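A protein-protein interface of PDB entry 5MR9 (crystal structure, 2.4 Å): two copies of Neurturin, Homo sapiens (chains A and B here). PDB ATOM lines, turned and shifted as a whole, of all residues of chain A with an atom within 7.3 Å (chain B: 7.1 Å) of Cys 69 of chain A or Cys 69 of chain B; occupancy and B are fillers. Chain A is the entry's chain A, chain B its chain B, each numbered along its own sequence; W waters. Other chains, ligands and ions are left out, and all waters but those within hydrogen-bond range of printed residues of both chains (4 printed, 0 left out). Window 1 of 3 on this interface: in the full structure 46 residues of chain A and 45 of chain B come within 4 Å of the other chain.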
ATOM      1  N   CYS A   8      36.082 -23.045  26.459  1.00  0.00           N
ATOM      2  CA  CYS A   8      34.824 -22.363  26.153  1.00  0.00           C
ATOM      3  C   CYS A   8      34.024 -22.121  27.446  1.00  0.00           C
ATOM      4  O   CYS A   8      33.795 -23.049  28.220  1.00  0.00           O
ATOM      5  CB  CYS A   8      34.027 -23.148  25.113  1.00  0.00           C
ATOM      6  SG  CYS A   8      32.401 -22.446  24.735  1.00  0.00           S
ATOM      7  N   GLY A  37      36.459 -18.996  24.056  1.00  0.00           N
ATOM      8  CA  GLY A  37      37.316 -20.093  24.483  1.00  0.00           C
ATOM      9  C   GLY A  37      37.634 -21.150  23.449  1.00  0.00           C
ATOM     10  O   GLY A  37      37.390 -20.961  22.256  1.00  0.00           O
ATOM     11  N   CYS A  39      37.540 -25.352  22.109  1.00  0.00           N
ATOM     12  CA  CYS A  39      36.677 -26.533  22.006  1.00  0.00           C
ATOM     13  C   CYS A  39      37.507 -27.799  21.701  1.00  0.00           C
ATOM     14  O   CYS A  39      37.272 -28.467  20.688  1.00  0.00           O
ATOM     15  CB  CYS A  39      35.577 -26.310  20.967  1.00  0.00           C
ATOM     16  SG  CYS A  39      34.587 -24.815  21.226  1.00  0.00           S
ATOM     17  N   ASP A  47      32.032 -35.522  13.571  1.00  0.00           N
ATOM     18  CA  ASP A  47      33.005 -34.571  13.013  1.00  0.00           C
ATOM     19  C   ASP A  47      34.096 -35.251  12.178  1.00  0.00           C
ATOM     20  O   ASP A  47      34.428 -34.764  11.094  1.00  0.00           O
ATOM     21  CB  ASP A  47      33.601 -33.625  14.095  1.00  0.00           C
ATOM     22  CG  ASP A  47      32.671 -32.523  14.569  1.00  0.00           C
ATOM     23  OD1 ASP A  47      31.768 -32.147  13.806  1.00  0.00           O
ATOM     24  OD2 ASP A  47      32.875 -32.014  15.700  1.00  0.00           O
ATOM     25  N   ARG A  65      30.401 -27.255   8.350  1.00  0.00           N
ATOM     26  CA  ARG A  65      31.158 -27.013   9.574  1.00  0.00           C
ATOM     27  C   ARG A  65      31.327 -28.358  10.273  1.00  0.00           C
ATOM     28  O   ARG A  65      30.349 -28.937  10.752  1.00  0.00           O
ATOM     29  CB  ARG A  65      30.456 -25.960  10.460  1.00  0.00           C
ATOM     30  CG  ARG A  65      31.088 -25.715  11.833  1.00  0.00           C
ATOM     31  CD  ARG A  65      32.433 -25.011  11.807  1.00  0.00           C
ATOM     32  NE  ARG A  65      32.971 -24.873  13.161  1.00  0.00           N
ATOM     33  CZ  ARG A  65      33.987 -24.083  13.495  1.00  0.00           C
ATOM     34  NH1 ARG A  65      34.595 -23.342  12.576  1.00  0.00           N
ATOM     35  NH2 ARG A  65      34.394 -24.015  14.757  1.00  0.00           N
ATOM     36  N   GLN A  67      33.515 -28.835  12.779  1.00  0.00           N
ATOM     37  CA  GLN A  67      34.254 -28.459  13.983  1.00  0.00           C
ATOM     38  C   GLN A  67      33.293 -27.898  15.035  1.00  0.00           C
ATOM     39  O   GLN A  67      32.394 -27.133  14.674  1.00  0.00           O
ATOM     40  CB  GLN A  67      35.312 -27.397  13.634  1.00  0.00           C
ATOM     41  CG  GLN A  67      36.737 -27.799  13.960  1.00  0.00           C
ATOM     42  CD  GLN A  67      37.732 -26.810  13.405  1.00  0.00           C
ATOM     43  OE1 GLN A  67      37.644 -25.598  13.629  1.00  0.00           O
ATOM     44  NE2 GLN A  67      38.700 -27.307  12.656  1.00  0.00           N
ATOM     45  N   PRO A  68      33.468 -28.230  16.338  1.00  0.00           N
ATOM     46  CA  PRO A  68      32.580 -27.647  17.370  1.00  0.00           C
ATOM     47  C   PRO A  68      32.743 -26.122  17.481  1.00  0.00           C
ATOM     48  O   PRO A  68      33.827 -25.596  17.222  1.00  0.00           O
ATOM     49  CB  PRO A  68      33.027 -28.355  18.656  1.00  0.00           C
ATOM     50  CG  PRO A  68      34.445 -28.734  18.406  1.00  0.00           C
ATOM     51  CD  PRO A  68      34.505 -29.096  16.945  1.00  0.00           C
ATOM     52  N   CYS A  69      31.668 -25.426  17.857  1.00  0.00           N
ATOM     53  CA  CYS A  69      31.664 -23.974  17.995  1.00  0.00           C
ATOM     54  C   CYS A  69      31.325 -23.541  19.408  1.00  0.00           C
ATOM     55  O   CYS A  69      30.354 -24.033  19.960  1.00  0.00           O
ATOM     56  CB  CYS A  69      30.721 -23.327  16.990  1.00  0.00           C
ATOM     57  SG  CYS A  69      31.100 -23.727  15.284  1.00  0.00           S
ATOM     58  N   CYS A  70      32.083 -22.588  19.958  1.00  0.00           N
ATOM     59  CA  CYS A  70      31.809 -22.039  21.289  1.00  0.00           C
ATOM     60  C   CYS A  70      30.731 -20.973  21.131  1.00  0.00           C
ATOM     61  O   CYS A  70      31.019 -19.853  20.675  1.00  0.00           O
ATOM     62  CB  CYS A  70      33.072 -21.484  21.936  1.00  0.00           C
ATOM     63  SG  CYS A  70      32.801 -20.813  23.583  1.00  0.00           S
ATOM     64  N   ARG A  71      29.478 -21.329  21.424  1.00  0.00           N
ATOM     65  CA  ARG A  71      28.328 -20.440  21.226  1.00  0.00           C
ATOM     66  C   ARG A  71      27.341 -20.474  22.403  1.00  0.00           C
ATOM     67  O   ARG A  71      27.324 -21.471  23.137  1.00  0.00           O
ATOM     68  CB  ARG A  71      27.599 -20.803  19.912  1.00  0.00           C
ATOM     69  CG  ARG A  71      28.341 -20.430  18.615  1.00  0.00           C
ATOM     70  CD  ARG A  71      28.290 -18.943  18.280  1.00  0.00           C
ATOM     71  NE  ARG A  71      26.920 -18.442  18.155  1.00  0.00           N
ATOM     72  CZ  ARG A  71      26.607 -17.179  17.887  1.00  0.00           C
ATOM     73  NH1 ARG A  71      27.561 -16.274  17.716  1.00  0.00           N
ATOM     74  NH2 ARG A  71      25.337 -16.812  17.785  1.00  0.00           N
ATOM     75  N   PRO A  72      26.488 -19.433  22.594  1.00  0.00           N
ATOM     76  CA  PRO A  72      25.498 -19.497  23.680  1.00  0.00           C
ATOM     77  C   PRO A  72      24.400 -20.529  23.447  1.00  0.00           C
ATOM     78  O   PRO A  72      23.853 -20.605  22.349  1.00  0.00           O
ATOM     79  CB  PRO A  72      24.917 -18.081  23.725  1.00  0.00           C
ATOM     80  CG  PRO A  72      25.802 -17.245  22.855  1.00  0.00           C
ATOM     81  CD  PRO A  72      26.366 -18.166  21.845  1.00  0.00           C
ATOM     82  N   CYS A  99      26.911 -21.219  27.927  1.00  0.00           N
ATOM     83  CA  CYS A  99      27.841 -21.452  26.821  1.00  0.00           C
ATOM     84  C   CYS A  99      28.071 -22.946  26.705  1.00  0.00           C
ATOM     85  O   CYS A  99      27.955 -23.665  27.693  1.00  0.00           O
ATOM     86  CB  CYS A  99      29.160 -20.712  27.032  1.00  0.00           C
ATOM     87  SG  CYS A  99      28.985 -18.929  27.133  1.00  0.00           S
ATOM     88  N   ALA A 100      28.438 -23.391  25.498  1.00  0.00           N
ATOM     89  CA  ALA A 100      28.786 -24.791  25.185  1.00  0.00           C
ATOM     90  C   ALA A 100      29.463 -24.887  23.837  1.00  0.00           C
ATOM     91  O   ALA A 100      29.493 -23.910  23.074  1.00  0.00           O
ATOM     92  CB  ALA A 100      27.545 -25.672  25.217  1.00  0.00           C
ATOM     93  N   CYS A 101      29.994 -26.064  23.546  1.00  0.00           N
ATOM     94  CA  CYS A 101      30.618 -26.375  22.269  1.00  0.00           C
ATOM     95  C   CYS A 101      29.549 -27.107  21.462  1.00  0.00           C
ATOM     96  O   CYS A 101      29.087 -28.174  21.881  1.00  0.00           O
ATOM     97  CB  CYS A 101      31.870 -27.228  22.456  1.00  0.00           C
ATOM     98  SG  CYS A 101      32.955 -26.661  23.788  1.00  0.00           S
ATOM     99  N   VAL A 102      29.092 -26.488  20.364  1.00  0.00           N
ATOM    100  CA  VAL A 102      28.073 -27.054  19.477  1.00  0.00           C
ATOM    101  C   VAL A 102      28.765 -27.434  18.166  1.00  0.00           C
ATOM    102  O   VAL A 102      29.099 -28.626  17.995  1.00  0.00           O
ATOM    103  CB  VAL A 102      26.804 -26.160  19.261  1.00  0.00           C
ATOM    104  CG1 VAL A 102      25.537 -27.009  19.240  1.00  0.00           C
ATOM    105  CG2 VAL A 102      26.684 -25.058  20.312  1.00  0.00           C
ATOM    106  OXT VAL A 102      29.105 -26.528  17.377  1.00  0.00           O
ATOM    107  N   CYS B   8      20.635 -23.513   6.481  1.00  0.00           N
ATOM    108  CA  CYS B   8      21.171 -24.567   7.323  1.00  0.00           C
ATOM    109  C   CYS B   8      20.087 -25.623   7.483  1.00  0.00           C
ATOM    110  O   CYS B   8      18.938 -25.289   7.786  1.00  0.00           O
ATOM    111  CB  CYS B   8      21.607 -23.997   8.670  1.00  0.00           C
ATOM    112  SG  CYS B   8      21.926 -25.254   9.933  1.00  0.00           S
ATOM    113  N   GLY B  37      24.915 -25.823   5.117  1.00  0.00           N
ATOM    114  CA  GLY B  37      24.189 -24.667   4.613  1.00  0.00           C
ATOM    115  C   GLY B  37      24.602 -23.347   5.233  1.00  0.00           C
ATOM    116  O   GLY B  37      25.457 -23.305   6.125  1.00  0.00           O
ATOM    117  N   CYS B  39      24.106 -19.671   7.280  1.00  0.00           N
ATOM    118  CA  CYS B  39      23.547 -19.172   8.531  1.00  0.00           C
ATOM    119  C   CYS B  39      23.601 -17.643   8.552  1.00  0.00           C
ATOM    120  O   CYS B  39      24.291 -17.059   9.395  1.00  0.00           O
ATOM    121  CB  CYS B  39      24.261 -19.767   9.742  1.00  0.00           C
ATOM    122  SG  CYS B  39      23.557 -21.319  10.358  1.00  0.00           S
ATOM    123  N   ARG B  65      33.399 -16.518  18.645  1.00  0.00           N
ATOM    124  CA  ARG B  65      32.564 -16.850  17.494  1.00  0.00           C
ATOM    125  C   ARG B  65      31.383 -15.889  17.505  1.00  0.00           C
ATOM    126  O   ARG B  65      30.433 -16.049  18.274  1.00  0.00           O
ATOM    127  CB  ARG B  65      32.151 -18.334  17.476  1.00  0.00           C
ATOM    128  CG  ARG B  65      32.221 -18.950  16.078  1.00  0.00           C
ATOM    129  CD  ARG B  65      32.904 -20.320  16.032  1.00  0.00           C
ATOM    130  NE  ARG B  65      34.355 -20.241  15.817  1.00  0.00           N
ATOM    131  CZ  ARG B  65      34.944 -20.053  14.639  1.00  0.00           C
ATOM    132  NH1 ARG B  65      34.208 -19.876  13.543  1.00  0.00           N
ATOM    133  NH2 ARG B  65      36.265 -19.998  14.546  1.00  0.00           N
ATOM    134  N   GLN B  67      29.446 -15.185  14.943  1.00  0.00           N
ATOM    135  CA  GLN B  67      28.459 -15.556  13.930  1.00  0.00           C
ATOM    136  C   GLN B  67      27.802 -16.885  14.250  1.00  0.00           C
ATOM    137  O   GLN B  67      28.482 -17.771  14.784  1.00  0.00           O
ATOM    138  CB  GLN B  67      29.112 -15.661  12.544  1.00  0.00           C
ATOM    139  CG  GLN B  67      29.017 -14.394  11.720  1.00  0.00           C
ATOM    140  CD  GLN B  67      30.380 -13.832  11.409  1.00  0.00           C
ATOM    141  OE1 GLN B  67      31.374 -14.558  11.298  1.00  0.00           O
ATOM    142  NE2 GLN B  67      30.456 -12.522  11.257  1.00  0.00           N
ATOM    143  N   PRO B  68      26.522 -17.093  13.848  1.00  0.00           N
ATOM    144  CA  PRO B  68      25.895 -18.406  14.075  1.00  0.00           C
ATOM    145  C   PRO B  68      26.533 -19.505  13.216  1.00  0.00           C
ATOM    146  O   PRO B  68      27.097 -19.225  12.152  1.00  0.00           O
ATOM    147  CB  PRO B  68      24.425 -18.176  13.688  1.00  0.00           C
ATOM    148  CG  PRO B  68      24.252 -16.700  13.592  1.00  0.00           C
ATOM    149  CD  PRO B  68      25.584 -16.170  13.176  1.00  0.00           C
ATOM    150  N   CYS B  69      26.445 -20.743  13.690  1.00  0.00           N
ATOM    151  CA  CYS B  69      27.011 -21.885  12.997  1.00  0.00           C
ATOM    152  C   CYS B  69      25.962 -22.964  12.746  1.00  0.00           C
ATOM    153  O   CYS B  69      25.149 -23.206  13.618  1.00  0.00           O
ATOM    154  CB  CYS B  69      28.210 -22.449  13.745  1.00  0.00           C
ATOM    155  SG  CYS B  69      29.513 -21.249  14.048  1.00  0.00           S
ATOM    156  N   CYS B  70      25.994 -23.585  11.561  1.00  0.00           N
ATOM    157  CA  CYS B  70      25.080 -24.674  11.229  1.00  0.00           C
ATOM    158  C   CYS B  70      25.630 -25.940  11.855  1.00  0.00           C
ATOM    159  O   CYS B  70      26.639 -26.482  11.381  1.00  0.00           O
ATOM    160  CB  CYS B  70      24.877 -24.811   9.728  1.00  0.00           C
ATOM    161  SG  CYS B  70      23.672 -26.067   9.284  1.00  0.00           S
ATOM    162  N   ARG B  71      25.068 -26.349  12.983  1.00  0.00           N
ATOM    163  CA  ARG B  71      25.565 -27.485  13.743  1.00  0.00           C
ATOM    164  C   ARG B  71      24.422 -28.345  14.253  1.00  0.00           C
ATOM    165  O   ARG B  71      23.311 -27.831  14.406  1.00  0.00           O
ATOM    166  CB  ARG B  71      26.449 -27.006  14.919  1.00  0.00           C
ATOM    167  CG  ARG B  71      27.829 -26.453  14.518  1.00  0.00           C
ATOM    168  CD  ARG B  71      28.818 -27.521  14.056  1.00  0.00           C
ATOM    169  NE  ARG B  71      29.183 -28.456  15.121  1.00  0.00           N
ATOM    170  CZ  ARG B  71      29.847 -29.594  14.936  1.00  0.00           C
ATOM    171  NH1 ARG B  71      30.225 -29.950  13.714  1.00  0.00           N
ATOM    172  NH2 ARG B  71      30.126 -30.379  15.959  1.00  0.00           N
ATOM    173  N   PRO B  72      24.647 -29.648  14.546  1.00  0.00           N
ATOM    174  CA  PRO B  72      23.558 -30.463  15.101  1.00  0.00           C
ATOM    175  C   PRO B  72      23.204 -30.076  16.539  1.00  0.00           C
ATOM    176  O   PRO B  72      24.098 -29.904  17.370  1.00  0.00           O
ATOM    177  CB  PRO B  72      24.106 -31.891  15.018  1.00  0.00           C
ATOM    178  CG  PRO B  72      25.342 -31.801  14.151  1.00  0.00           C
ATOM    179  CD  PRO B  72      25.879 -30.444  14.417  1.00  0.00           C
ATOM    180  N   ALA B 100      20.379 -26.562  13.452  1.00  0.00           N
ATOM    181  CA  ALA B 100      20.019 -25.178  13.836  1.00  0.00           C
ATOM    182  C   ALA B 100      21.206 -24.247  13.664  1.00  0.00           C
ATOM    183  O   ALA B 100      22.351 -24.707  13.681  1.00  0.00           O
ATOM    184  CB  ALA B 100      19.525 -25.137  15.275  1.00  0.00           C
ATOM    185  N   CYS B 101      20.932 -22.944  13.514  1.00  0.00           N
ATOM    186  CA  CYS B 101      21.963 -21.915  13.437  1.00  0.00           C
ATOM    187  C   CYS B 101      22.252 -21.494  14.874  1.00  0.00           C
ATOM    188  O   CYS B 101      21.459 -20.775  15.489  1.00  0.00           O
ATOM    189  CB  CYS B 101      21.525 -20.734  12.574  1.00  0.00           C
ATOM    190  SG  CYS B 101      21.577 -21.060  10.791  1.00  0.00           S
ATOM    191  N   VAL B 102      23.349 -22.028  15.432  1.00  0.00           N
ATOM    192  CA  VAL B 102      23.778 -21.780  16.812  1.00  0.00           C
ATOM    193  C   VAL B 102      24.507 -20.431  16.990  1.00  0.00           C
ATOM    194  O   VAL B 102      24.004 -19.558  17.722  1.00  0.00           O
ATOM    195  CB  VAL B 102      24.497 -22.999  17.489  1.00  0.00           C
ATOM    196  CG1 VAL B 102      23.658 -24.271  17.373  1.00  0.00           C
ATOM    197  CG2 VAL B 102      25.910 -23.233  16.940  1.00  0.00           C
ATOM    198  OXT VAL B 102      25.575 -20.226  16.390  1.00  0.00           O
HETATM  199  O   HOH W   1      29.749 -16.662  21.078  1.00  0.00           O
HETATM  200  O   HOH W   2      26.752 -30.252  18.070  1.00  0.00           O
HETATM  201  O   HOH W   3      27.807 -29.725  10.981  1.00  0.00           O
HETATM  202  O   HOH W   4      27.603 -27.104   8.981  1.00  0.00           O
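Cys 69 of chain A touches just these residues of chain B: Arg 65 and Cys 69.
Cys 69 of chain B touches one residue of chain A.
Of the printed residues of chain B, Gln 67 of chain A touches Arg 71 (3.5 Å).
Of the printed residues of chain A, Arg 71 of chain B touches Asp 47 (2.7 Å), Arg 65 (3.1 Å), Gln 67 (3.5 Å), Pro 68 (3.9 Å) and Val 102 (2.9 Å).
Of the printed residues of chain A, Cys 70 of chain B touches Arg 65.
Of the printed residues of chain B, Cys 70 of chain A touches Arg 65 (3.7 Å).
Of the printed residues of chain B, Val 102 of chain A touches Arg 71 (2.9 Å), Pro 72 (3.7 Å) and Val 102 (3.8 Å).
Cys 99 of chain A touches none of the printed residues of chain B.
The nearest residue of chain B that does not touch Cys 69 of chain A is Arg 71 of chain B (4.3 Å).
The nearest printed residue of chain A that does not touch Val 102 of chain B is Pro 72 of chain A (4.7 Å).
The backbone carbonyl oxygen (O) of Gln 67 of chain B sits at hydrogen-bond distance from the side-chain sulfur (SG) of Cys 69 of chain B, 3.7 Å away.
SG of Cys 39 of chain B is disulfide-bonded to SG of Cys 101 of chain B.
N of Cys 70 of chain A is in hydrogen-bond range of SG of Cys 39 of chain A.
The backbone carbonyl oxygen (O) of Pro 68 of chain A sits at hydrogen-bond distance from the guanidinium group (NH2) of Arg 65 of chain A.
The backbone carbonyl oxygen (O) of Gln 67 of chain A is in hydrogen-bond range of the guanidinium group (NE) of Arg 65 of chain A (2.8 Å).
The guanidinium group (NE) of Arg 65 of chain A is in hydrogen-bond range of the side-chain sulfur (SG) of Cys 69 of chain A, 3.1 Å away.
Of the 13 printed residues of chain B, 7 touch a printed residue of chain A.
Printed residues of chain B that touch a printed residue of chain A: Arg 65, Gln 67, Cys 69, Cys 70, Arg 71, Pro 72 and Val 102.
Along chain B the printed residues that touch a printed residue of chain A span positions 65 to 102.
Printed residues of chain A that touch a printed residue of chain B: Asp 47, Arg 65, Gln 67, Pro 68, Cys 69, Cys 70, Arg 71 and Val 102.
Hydrophobic or aromatic side chains of chain A that line the printed part of chain B: Val 102.
Among the printed residues, 15 pairs touch across the chains.
Water W4 lies within hydrogen-bond range of the backbone carbonyl oxygen of Cys 70 of chain B and the backbone NH of Arg 65 of chain A.
Water W3 bridges the backbone carbonyl oxygen (O) of Arg 65 of chain A and the backbone carbonyl oxygen (O) of Cys 70 of chain B.
Water W2 lies within hydrogen-bond range of the backbone carbonyl oxygen of Pro 72 of chain B (2.8 Å) and the chain-end carboxylate of Val 102 of chain A (2.9 Å).
Water W1 lies within hydrogen-bond range of O of Arg 65 of chain B (3.0 Å) and O of Cys 70 of chain A (3.5 Å).
Arg 65 of chain A touches Arg 65 of chain B.
Cys 70 of chain B touches Arg 65 of chain A.
Arg 71 of chain B touches Gln 67 of chain A.
Pro 68 of chain A touches Arg 71 of chain B (CA to NH2, 3.9 Å).
CB of Cys 69 of chain A touches CD of Arg 65 of chain B (3.8 Å).
Arg 65 of chain B touches Cys 70 of chain A (CB to O, 3.7 Å).
Val 102 of chain A touches Pro 72 of chain B (CG1 to O, 3.7 Å).
Val 102 of chain B touches Val 102 of chain A.
Gln 67 of chain A touches Arg 71 of chain B, and with the chains exchanged Arg 71 of chain A touches Gln 67 of chain B.
Pro 68 of chain A touches Arg 71 of chain B, but with the chains exchanged Arg 71 of chain A does not touch Pro 68 of chain B (4.04 Å).
Arg 71 of chain A touches Val 102 of chain B, and with the chains exchanged Val 102 of chain A touches Arg 71 of chain B.
Val 102 of chain A touches its own counterpart, Val 102 of chain B.
13 positions are printed for both chains.
Of the 15 pairs that touch across the chains among the printed residues, 11 have their exchanged pair printed and touching as well.
NH1 of Arg 71 of chain A lies within hydrogen-bond range of O of Arg 65 of chain B (2.9 Å).
The side-chain sulfur (SG) of Cys 69 of chain A lies close to the side-chain sulfur (SG) of Cys 69 of chain B (3.2 Å).
The guanidinium group (NE) of Arg 71 of chain A lies within salt-bridge range of the chain-end carboxylate (OXT) of Val 102 of chain B, at 2.8 Å.
The backbone carbonyl oxygen of Arg 65 of chain A is in hydrogen-bond range of the guanidinium group of Arg 71 of chain B.
NH1 of Arg 71 of chain A lies within hydrogen-bond range of O of Gln 67 of chain B (3.4 Å).
The side-chain carboxylate (OD1) of Asp 47 of chain A lies within salt-bridge range of the guanidinium group (NH1) of Arg 71 of chain B (2.7 Å).
The guanidinium group of Arg 71 of chain B lies within salt-bridge range of the chain-end carboxylate of Val 102 of chain A (2.9 Å).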
